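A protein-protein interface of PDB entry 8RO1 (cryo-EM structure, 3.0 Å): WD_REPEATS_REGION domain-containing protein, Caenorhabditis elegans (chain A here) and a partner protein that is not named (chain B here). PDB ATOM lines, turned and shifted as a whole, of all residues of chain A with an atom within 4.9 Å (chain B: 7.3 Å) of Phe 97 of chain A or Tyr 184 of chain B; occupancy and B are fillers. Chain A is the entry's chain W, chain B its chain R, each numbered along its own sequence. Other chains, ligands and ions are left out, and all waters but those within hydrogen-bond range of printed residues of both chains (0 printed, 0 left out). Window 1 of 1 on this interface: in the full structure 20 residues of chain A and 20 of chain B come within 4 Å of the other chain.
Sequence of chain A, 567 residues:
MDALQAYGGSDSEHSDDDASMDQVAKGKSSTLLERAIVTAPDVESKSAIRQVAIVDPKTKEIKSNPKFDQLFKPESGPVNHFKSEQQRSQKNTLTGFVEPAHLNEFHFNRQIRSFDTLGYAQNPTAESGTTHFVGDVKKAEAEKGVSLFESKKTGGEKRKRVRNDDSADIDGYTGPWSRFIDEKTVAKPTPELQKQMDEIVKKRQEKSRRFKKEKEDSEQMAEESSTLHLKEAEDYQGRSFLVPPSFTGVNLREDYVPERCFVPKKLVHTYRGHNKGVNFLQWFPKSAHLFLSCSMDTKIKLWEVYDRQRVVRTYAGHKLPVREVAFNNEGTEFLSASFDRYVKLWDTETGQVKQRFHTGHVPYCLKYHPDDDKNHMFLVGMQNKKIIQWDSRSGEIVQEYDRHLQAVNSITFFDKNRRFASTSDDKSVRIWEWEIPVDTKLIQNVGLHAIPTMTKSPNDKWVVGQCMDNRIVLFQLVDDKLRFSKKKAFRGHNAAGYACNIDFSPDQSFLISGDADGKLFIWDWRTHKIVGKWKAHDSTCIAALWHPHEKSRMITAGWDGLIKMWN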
ATOM      1  N   GLN A  90      20.590  21.969 -12.170  1.00  0.00           N
ATOM      2  CA  GLN A  90      20.558  23.410 -11.986  1.00  0.00           C
ATOM      3  C   GLN A  90      20.900  23.722 -10.547  1.00  0.00           C
ATOM      4  O   GLN A  90      20.382  23.080  -9.628  1.00  0.00           O
ATOM      5  CB  GLN A  90      19.158  23.935 -12.313  1.00  0.00           C
ATOM      6  CG  GLN A  90      18.893  25.440 -12.132  1.00  0.00           C
ATOM      7  CD  GLN A  90      19.570  26.323 -13.140  1.00  0.00           C
ATOM      8  OE1 GLN A  90      20.626  25.995 -13.669  1.00  0.00           O
ATOM      9  NE2 GLN A  90      18.964  27.476 -13.404  1.00  0.00           N
ATOM     10  N   LYS A  91      21.761  24.706 -10.341  1.00  0.00           N
ATOM     11  CA  LYS A  91      22.056  25.115  -8.979  1.00  0.00           C
ATOM     12  C   LYS A  91      22.521  26.559  -8.971  1.00  0.00           C
ATOM     13  O   LYS A  91      22.821  27.151 -10.007  1.00  0.00           O
ATOM     14  CB  LYS A  91      23.027  24.112  -8.334  1.00  0.00           C
ATOM     15  CG  LYS A  91      24.494  24.220  -8.637  1.00  0.00           C
ATOM     16  CD  LYS A  91      25.200  23.106  -7.897  1.00  0.00           C
ATOM     17  CE  LYS A  91      26.684  23.152  -8.030  1.00  0.00           C
ATOM     18  NZ  LYS A  91      27.107  22.974  -9.440  1.00  0.00           N
ATOM     19  N   ASN A  92      22.578  27.105  -7.763  1.00  0.00           N
ATOM     20  CA  ASN A  92      22.947  28.483  -7.503  1.00  0.00           C
ATOM     21  C   ASN A  92      23.747  28.689  -6.236  1.00  0.00           C
ATOM     22  O   ASN A  92      24.869  29.191  -6.303  1.00  0.00           O
ATOM     23  CB  ASN A  92      21.660  29.285  -7.388  1.00  0.00           C
ATOM     24  CG  ASN A  92      21.901  30.738  -7.249  1.00  0.00           C
ATOM     25  OD1 ASN A  92      22.780  31.305  -7.891  1.00  0.00           O
ATOM     26  ND2 ASN A  92      21.125  31.369  -6.379  1.00  0.00           N
ATOM     27  N   THR A  95      24.956  23.704  -3.188  1.00  0.00           N
ATOM     28  CA  THR A  95      24.262  22.463  -3.530  1.00  0.00           C
ATOM     29  C   THR A  95      22.997  22.553  -4.377  1.00  0.00           C
ATOM     30  O   THR A  95      22.486  21.502  -4.767  1.00  0.00           O
ATOM     31  CB  THR A  95      23.863  21.743  -2.232  1.00  0.00           C
ATOM     32  OG1 THR A  95      22.867  22.516  -1.561  1.00  0.00           O
ATOM     33  CG2 THR A  95      25.032  21.534  -1.301  1.00  0.00           C
ATOM     34  N   GLY A  96      22.454  23.724  -4.662  1.00  0.00           N
ATOM     35  CA  GLY A  96      21.019  23.776  -4.875  1.00  0.00           C
ATOM     36  C   GLY A  96      20.627  25.095  -5.481  1.00  0.00           C
ATOM     37  O   GLY A  96      21.424  26.034  -5.526  1.00  0.00           O
ATOM     38  N   PHE A  97      19.408  25.143  -6.009  1.00  0.00           N
ATOM     39  CA  PHE A  97      18.791  26.410  -6.378  1.00  0.00           C
ATOM     40  C   PHE A  97      17.930  26.857  -5.206  1.00  0.00           C
ATOM     41  O   PHE A  97      16.924  26.218  -4.896  1.00  0.00           O
ATOM     42  CB  PHE A  97      17.992  26.318  -7.668  1.00  0.00           C
ATOM     43  CG  PHE A  97      17.802  27.644  -8.302  1.00  0.00           C
ATOM     44  CD1 PHE A  97      16.787  28.484  -7.940  1.00  0.00           C
ATOM     45  CD2 PHE A  97      18.678  28.054  -9.260  1.00  0.00           C
ATOM     46  CE1 PHE A  97      16.653  29.705  -8.539  1.00  0.00           C
ATOM     47  CE2 PHE A  97      18.551  29.258  -9.860  1.00  0.00           C
ATOM     48  CZ  PHE A  97      17.557  30.103  -9.486  1.00  0.00           C
ATOM     49  N   VAL A  98      18.326  27.932  -4.553  1.00  0.00           N
ATOM     50  CA  VAL A  98      17.602  28.518  -3.432  1.00  0.00           C
ATOM     51  C   VAL A  98      16.910  29.767  -3.939  1.00  0.00           C
ATOM     52  O   VAL A  98      17.563  30.650  -4.506  1.00  0.00           O
ATOM     53  CB  VAL A  98      18.536  28.820  -2.251  1.00  0.00           C
ATOM     54  CG1 VAL A  98      17.803  29.515  -1.132  1.00  0.00           C
ATOM     55  CG2 VAL A  98      19.113  27.519  -1.702  1.00  0.00           C
ATOM     56  N   GLU A  99      15.595  29.831  -3.755  1.00  0.00           N
ATOM     57  CA  GLU A  99      14.795  30.979  -4.146  1.00  0.00           C
ATOM     58  C   GLU A  99      13.707  31.194  -3.107  1.00  0.00           C
ATOM     59  O   GLU A  99      13.163  30.219  -2.581  1.00  0.00           O
ATOM     60  CB  GLU A  99      14.141  30.780  -5.519  1.00  0.00           C
ATOM     61  CG  GLU A  99      13.175  29.621  -5.580  1.00  0.00           C
ATOM     62  CD  GLU A  99      12.773  29.288  -6.981  1.00  0.00           C
ATOM     63  OE1 GLU A  99      12.809  30.190  -7.838  1.00  0.00           O
ATOM     64  OE2 GLU A  99      12.417  28.119  -7.230  1.00  0.00           O
ATOM     65  N   ILE B 182      11.318  29.379   1.690  1.00  0.00           N
ATOM     66  CA  ILE B 182      12.353  29.143   0.701  1.00  0.00           C
ATOM     67  C   ILE B 182      11.853  27.945  -0.085  1.00  0.00           C
ATOM     68  O   ILE B 182      11.349  26.996   0.517  1.00  0.00           O
ATOM     69  CB  ILE B 182      13.720  28.911   1.374  1.00  0.00           C
ATOM     70  CG1 ILE B 182      14.252  30.278   1.819  1.00  0.00           C
ATOM     71  CG2 ILE B 182      14.700  28.196   0.435  1.00  0.00           C
ATOM     72  CD1 ILE B 182      15.602  30.304   2.467  1.00  0.00           C
ATOM     73  N   ARG B 183      12.024  27.956  -1.404  1.00  0.00           N
ATOM     74  CA  ARG B 183      11.907  26.728  -2.174  1.00  0.00           C
ATOM     75  C   ARG B 183      13.305  26.369  -2.625  1.00  0.00           C
ATOM     76  O   ARG B 183      13.964  27.146  -3.316  1.00  0.00           O
ATOM     77  CB  ARG B 183      10.960  26.965  -3.357  1.00  0.00           C
ATOM     78  CG  ARG B 183      10.366  25.760  -4.065  1.00  0.00           C
ATOM     79  CD  ARG B 183       9.305  26.188  -5.093  1.00  0.00           C
ATOM     80  NE  ARG B 183       9.878  26.857  -6.257  1.00  0.00           N
ATOM     81  CZ  ARG B 183       9.230  27.122  -7.390  1.00  0.00           C
ATOM     82  NH1 ARG B 183       9.895  27.663  -8.408  1.00  0.00           N
ATOM     83  NH2 ARG B 183       7.927  26.918  -7.513  1.00  0.00           N
ATOM     84  N   TYR B 184      13.714  25.169  -2.258  1.00  0.00           N
ATOM     85  CA  TYR B 184      15.075  24.687  -2.397  1.00  0.00           C
ATOM     86  C   TYR B 184      15.005  23.563  -3.402  1.00  0.00           C
ATOM     87  O   TYR B 184      14.277  22.596  -3.170  1.00  0.00           O
ATOM     88  CB  TYR B 184      15.635  24.271  -1.042  1.00  0.00           C
ATOM     89  CG  TYR B 184      16.894  23.466  -1.030  1.00  0.00           C
ATOM     90  CD1 TYR B 184      18.036  23.940  -1.635  1.00  0.00           C
ATOM     91  CD2 TYR B 184      16.976  22.291  -0.344  1.00  0.00           C
ATOM     92  CE1 TYR B 184      19.180  23.231  -1.615  1.00  0.00           C
ATOM     93  CE2 TYR B 184      18.128  21.588  -0.303  1.00  0.00           C
ATOM     94  CZ  TYR B 184      19.226  22.070  -0.929  1.00  0.00           C
ATOM     95  OH  TYR B 184      20.393  21.361  -0.846  1.00  0.00           O
ATOM     96  N   THR B 185      15.749  23.673  -4.491  1.00  0.00           N
ATOM     97  CA  THR B 185      15.849  22.561  -5.410  1.00  0.00           C
ATOM     98  C   THR B 185      17.231  21.948  -5.268  1.00  0.00           C
ATOM     99  O   THR B 185      18.220  22.611  -5.599  1.00  0.00           O
ATOM    100  CB  THR B 185      15.647  23.063  -6.835  1.00  0.00           C
ATOM    101  OG1 THR B 185      14.448  23.836  -6.910  1.00  0.00           O
ATOM    102  CG2 THR B 185      15.557  21.936  -7.815  1.00  0.00           C
ATOM    103  N   PRO B 186      17.356  20.674  -4.833  1.00  0.00           N
ATOM    104  CA  PRO B 186      18.656  20.167  -4.413  1.00  0.00           C
ATOM    105  C   PRO B 186      19.241  19.404  -5.566  1.00  0.00           C
ATOM    106  O   PRO B 186      18.577  18.509  -6.091  1.00  0.00           O
ATOM    107  CB  PRO B 186      18.338  19.240  -3.246  1.00  0.00           C
ATOM    108  CG  PRO B 186      17.016  18.816  -3.461  1.00  0.00           C
ATOM    109  CD  PRO B 186      16.303  19.873  -4.188  1.00  0.00           C
ATOM    110  N   SER B 187      20.455  19.739  -5.986  1.00  0.00           N
ATOM    111  CA  SER B 187      21.052  18.968  -7.061  1.00  0.00           C
ATOM    112  C   SER B 187      21.308  17.532  -6.638  1.00  0.00           C
ATOM    113  O   SER B 187      21.363  16.643  -7.491  1.00  0.00           O
ATOM    114  CB  SER B 187      22.345  19.641  -7.496  1.00  0.00           C
ATOM    115  OG  SER B 187      23.285  19.618  -6.444  1.00  0.00           O
ATOM    116  N   GLN B 188      21.488  17.276  -5.351  1.00  0.00           N
ATOM    117  CA  GLN B 188      21.613  15.904  -4.879  1.00  0.00           C
ATOM    118  C   GLN B 188      20.265  15.230  -5.098  1.00  0.00           C
ATOM    119  O   GLN B 188      19.372  15.315  -4.257  1.00  0.00           O
ATOM    120  CB  GLN B 188      22.059  15.876  -3.427  1.00  0.00           C
ATOM    121  CG  GLN B 188      22.458  14.486  -2.973  1.00  0.00           C
ATOM    122  CD  GLN B 188      23.005  14.403  -1.555  1.00  0.00           C
ATOM    123  OE1 GLN B 188      22.841  13.376  -0.899  1.00  0.00           O
ATOM    124  NE2 GLN B 188      23.710  15.442  -1.096  1.00  0.00           N
ATOM    125  N   SER B 195      10.325  14.088  -4.386  1.00  0.00           N
ATOM    126  CA  SER B 195      10.245  15.531  -4.598  1.00  0.00           C
ATOM    127  C   SER B 195      11.556  16.096  -5.105  1.00  0.00           C
ATOM    128  O   SER B 195      12.582  16.013  -4.429  1.00  0.00           O
ATOM    129  CB  SER B 195       9.841  16.250  -3.319  1.00  0.00           C
ATOM    130  OG  SER B 195       8.635  15.723  -2.812  1.00  0.00           O
ATOM    131  N   GLN B 196      11.511  16.666  -6.300  1.00  0.00           N
ATOM    132  CA  GLN B 196      12.664  17.332  -6.876  1.00  0.00           C
ATOM    133  C   GLN B 196      12.968  18.652  -6.193  1.00  0.00           C
ATOM    134  O   GLN B 196      13.981  19.264  -6.524  1.00  0.00           O
ATOM    135  CB  GLN B 196      12.462  17.591  -8.366  1.00  0.00           C
ATOM    136  CG  GLN B 196      12.380  16.349  -9.212  1.00  0.00           C
ATOM    137  CD  GLN B 196      10.988  15.755  -9.267  1.00  0.00           C
ATOM    138  OE1 GLN B 196      10.087  16.179  -8.546  1.00  0.00           O
ATOM    139  NE2 GLN B 196      10.810  14.754 -10.117  1.00  0.00           N
ATOM    140  N   GLN B 197      12.091  19.144  -5.324  1.00  0.00           N
ATOM    141  CA  GLN B 197      12.341  20.328  -4.527  1.00  0.00           C
ATOM    142  C   GLN B 197      11.815  20.116  -3.125  1.00  0.00           C
ATOM    143  O   GLN B 197      11.040  19.203  -2.849  1.00  0.00           O
ATOM    144  CB  GLN B 197      11.688  21.603  -5.066  1.00  0.00           C
ATOM    145  CG  GLN B 197      11.588  21.773  -6.537  1.00  0.00           C
ATOM    146  CD  GLN B 197      10.855  23.046  -6.872  1.00  0.00           C
ATOM    147  OE1 GLN B 197       9.652  23.142  -6.671  1.00  0.00           O
ATOM    148  NE2 GLN B 197      11.572  24.031  -7.389  1.00  0.00           N
ATOM    149  N   ARG B 198      12.263  20.994  -2.250  1.00  0.00           N
ATOM    150  CA  ARG B 198      11.730  21.127  -0.914  1.00  0.00           C
ATOM    151  C   ARG B 198      11.216  22.539  -0.821  1.00  0.00           C
ATOM    152  O   ARG B 198      11.720  23.439  -1.494  1.00  0.00           O
ATOM    153  CB  ARG B 198      12.787  20.945   0.140  1.00  0.00           C
ATOM    154  CG  ARG B 198      13.423  19.627   0.151  1.00  0.00           C
ATOM    155  CD  ARG B 198      14.619  19.632   1.038  1.00  0.00           C
ATOM    156  NE  ARG B 198      15.157  18.289   1.109  1.00  0.00           N
ATOM    157  CZ  ARG B 198      14.753  17.354   1.950  1.00  0.00           C
ATOM    158  NH1 ARG B 198      15.188  16.121   1.784  1.00  0.00           N
ATOM    159  NH2 ARG B 198      13.899  17.605   2.929  1.00  0.00           N
ATOM    160  N   ILE B 199      10.227  22.724   0.028  1.00  0.00           N
ATOM    161  CA  ILE B 199       9.799  24.038   0.455  1.00  0.00           C
ATOM    162  C   ILE B 199       9.813  24.052   1.963  1.00  0.00           C
ATOM    163  O   ILE B 199       9.411  23.077   2.601  1.00  0.00           O
ATOM    164  CB  ILE B 199       8.427  24.391  -0.158  1.00  0.00           C
ATOM    165  CG1 ILE B 199       8.144  25.888  -0.047  1.00  0.00           C
ATOM    166  CG2 ILE B 199       7.313  23.588   0.460  1.00  0.00           C
ATOM    167  CD1 ILE B 199       7.482  26.460  -1.291  1.00  0.00           C
ATOM    168  N   ILE B 200      10.299  25.149   2.528  1.00  0.00           N
ATOM    169  CA  ILE B 200      10.825  25.146   3.877  1.00  0.00           C
ATOM    170  C   ILE B 200      10.567  26.513   4.477  1.00  0.00           C
ATOM    171  O   ILE B 200      10.606  27.533   3.790  1.00  0.00           O
ATOM    172  CB  ILE B 200      12.337  24.771   3.874  1.00  0.00           C
ATOM    173  CG1 ILE B 200      13.079  25.333   5.087  1.00  0.00           C
ATOM    174  CG2 ILE B 200      13.020  25.186   2.580  1.00  0.00           C
ATOM    175  CD1 ILE B 200      14.346  24.647   5.396  1.00  0.00           C
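Of the printed residues of chain B, Phe 97 of chain A touches Arg 183 (3.5 Å), Tyr 184 (3.5 Å) and Thr 185 (2.8 Å).
Printed residues of chain A within 4 Å of Thr 185 of chain B: Gly 96 (3.1 Å) and Phe 97 (2.8 Å).
Of the printed residues of chain B, Thr 95 of chain A touches Tyr 184, Pro 186 and Ser 187.
Printed residues of chain B within 4 Å of Gly 96 of chain A: Tyr 184 and Thr 185.
Gln 196 of chain B touches none of the printed residues of chain A.
The nearest residue of chain B that does not touch Phe 97 of chain A is Pro 186 of chain B (5.1 Å).
O of Ile 200 of chain B sits at hydrogen-bond distance from N of Ile 182 of chain B, 2.9 Å away.
The side-chain amide nitrogen (NE2) of Gln 197 of chain B sits close to the guanidinium group (NE) of Arg 183 of chain B (3.5 Å).
The backbone carbonyl oxygen of Tyr 184 of chain B lies within hydrogen-bond range of the backbone NH of Arg 198 of chain B.
The side-chain amide nitrogen (NE2) of Gln 197 of chain B is in hydrogen-bond range of the side-chain hydroxyl (OG1) of Thr 185 of chain B, 2.9 Å away.
Hydrophobic or aromatic side chains of chain B that line the printed part of chain A: Ile 182 and Tyr 184.
Among the printed residues, 13 pairs touch across the chains.
The side-chain carboxylate (OE2) of Glu 99 of chain A is in salt-bridge range of the guanidinium group (NH1) of Arg 183 of chain B (2.8 Å).
OH of Tyr 184 of chain B is in hydrogen-bond range of OG1 of Thr 95 of chain A (2.8 Å).
The backbone NH of Phe 97 of chain A sits at hydrogen-bond distance from the backbone carbonyl oxygen of Thr 185 of chain B, 2.8 Å away.
The side-chain hydroxyl (OG) of Ser 187 of chain B sits at hydrogen-bond distance from the backbone carbonyl oxygen (O) of Thr 95 of chain A, 2.6 Å away.
The backbone carbonyl oxygen of Arg 183 of chain B lies close to the backbone carbonyl oxygen of Phe 97 of chain A (3.5 Å).
Thr 95 of chain A touches Pro 186 of chain B.
Gly 96 of chain A touches Tyr 184 of chain B (CA to CE1, 3.8 Å).
CA of Gly 96 of chain A touches O of Thr 185 of chain B, at 3.1 Å.
O of Phe 97 of chain A touches CA of Tyr 184 of chain B, at 3.5 Å.
Ile 182 of chain B touches Val 98 of chain A (CG2 to CG1, 3.7 Å).
Val 98 of chain A touches Arg 183 of chain B.
CD1 of Tyr 184 of chain B touches CG2 of Val 98 of chain A, 3.7 Å away.
Glu 99 of chain A touches Ile 182 of chain B.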
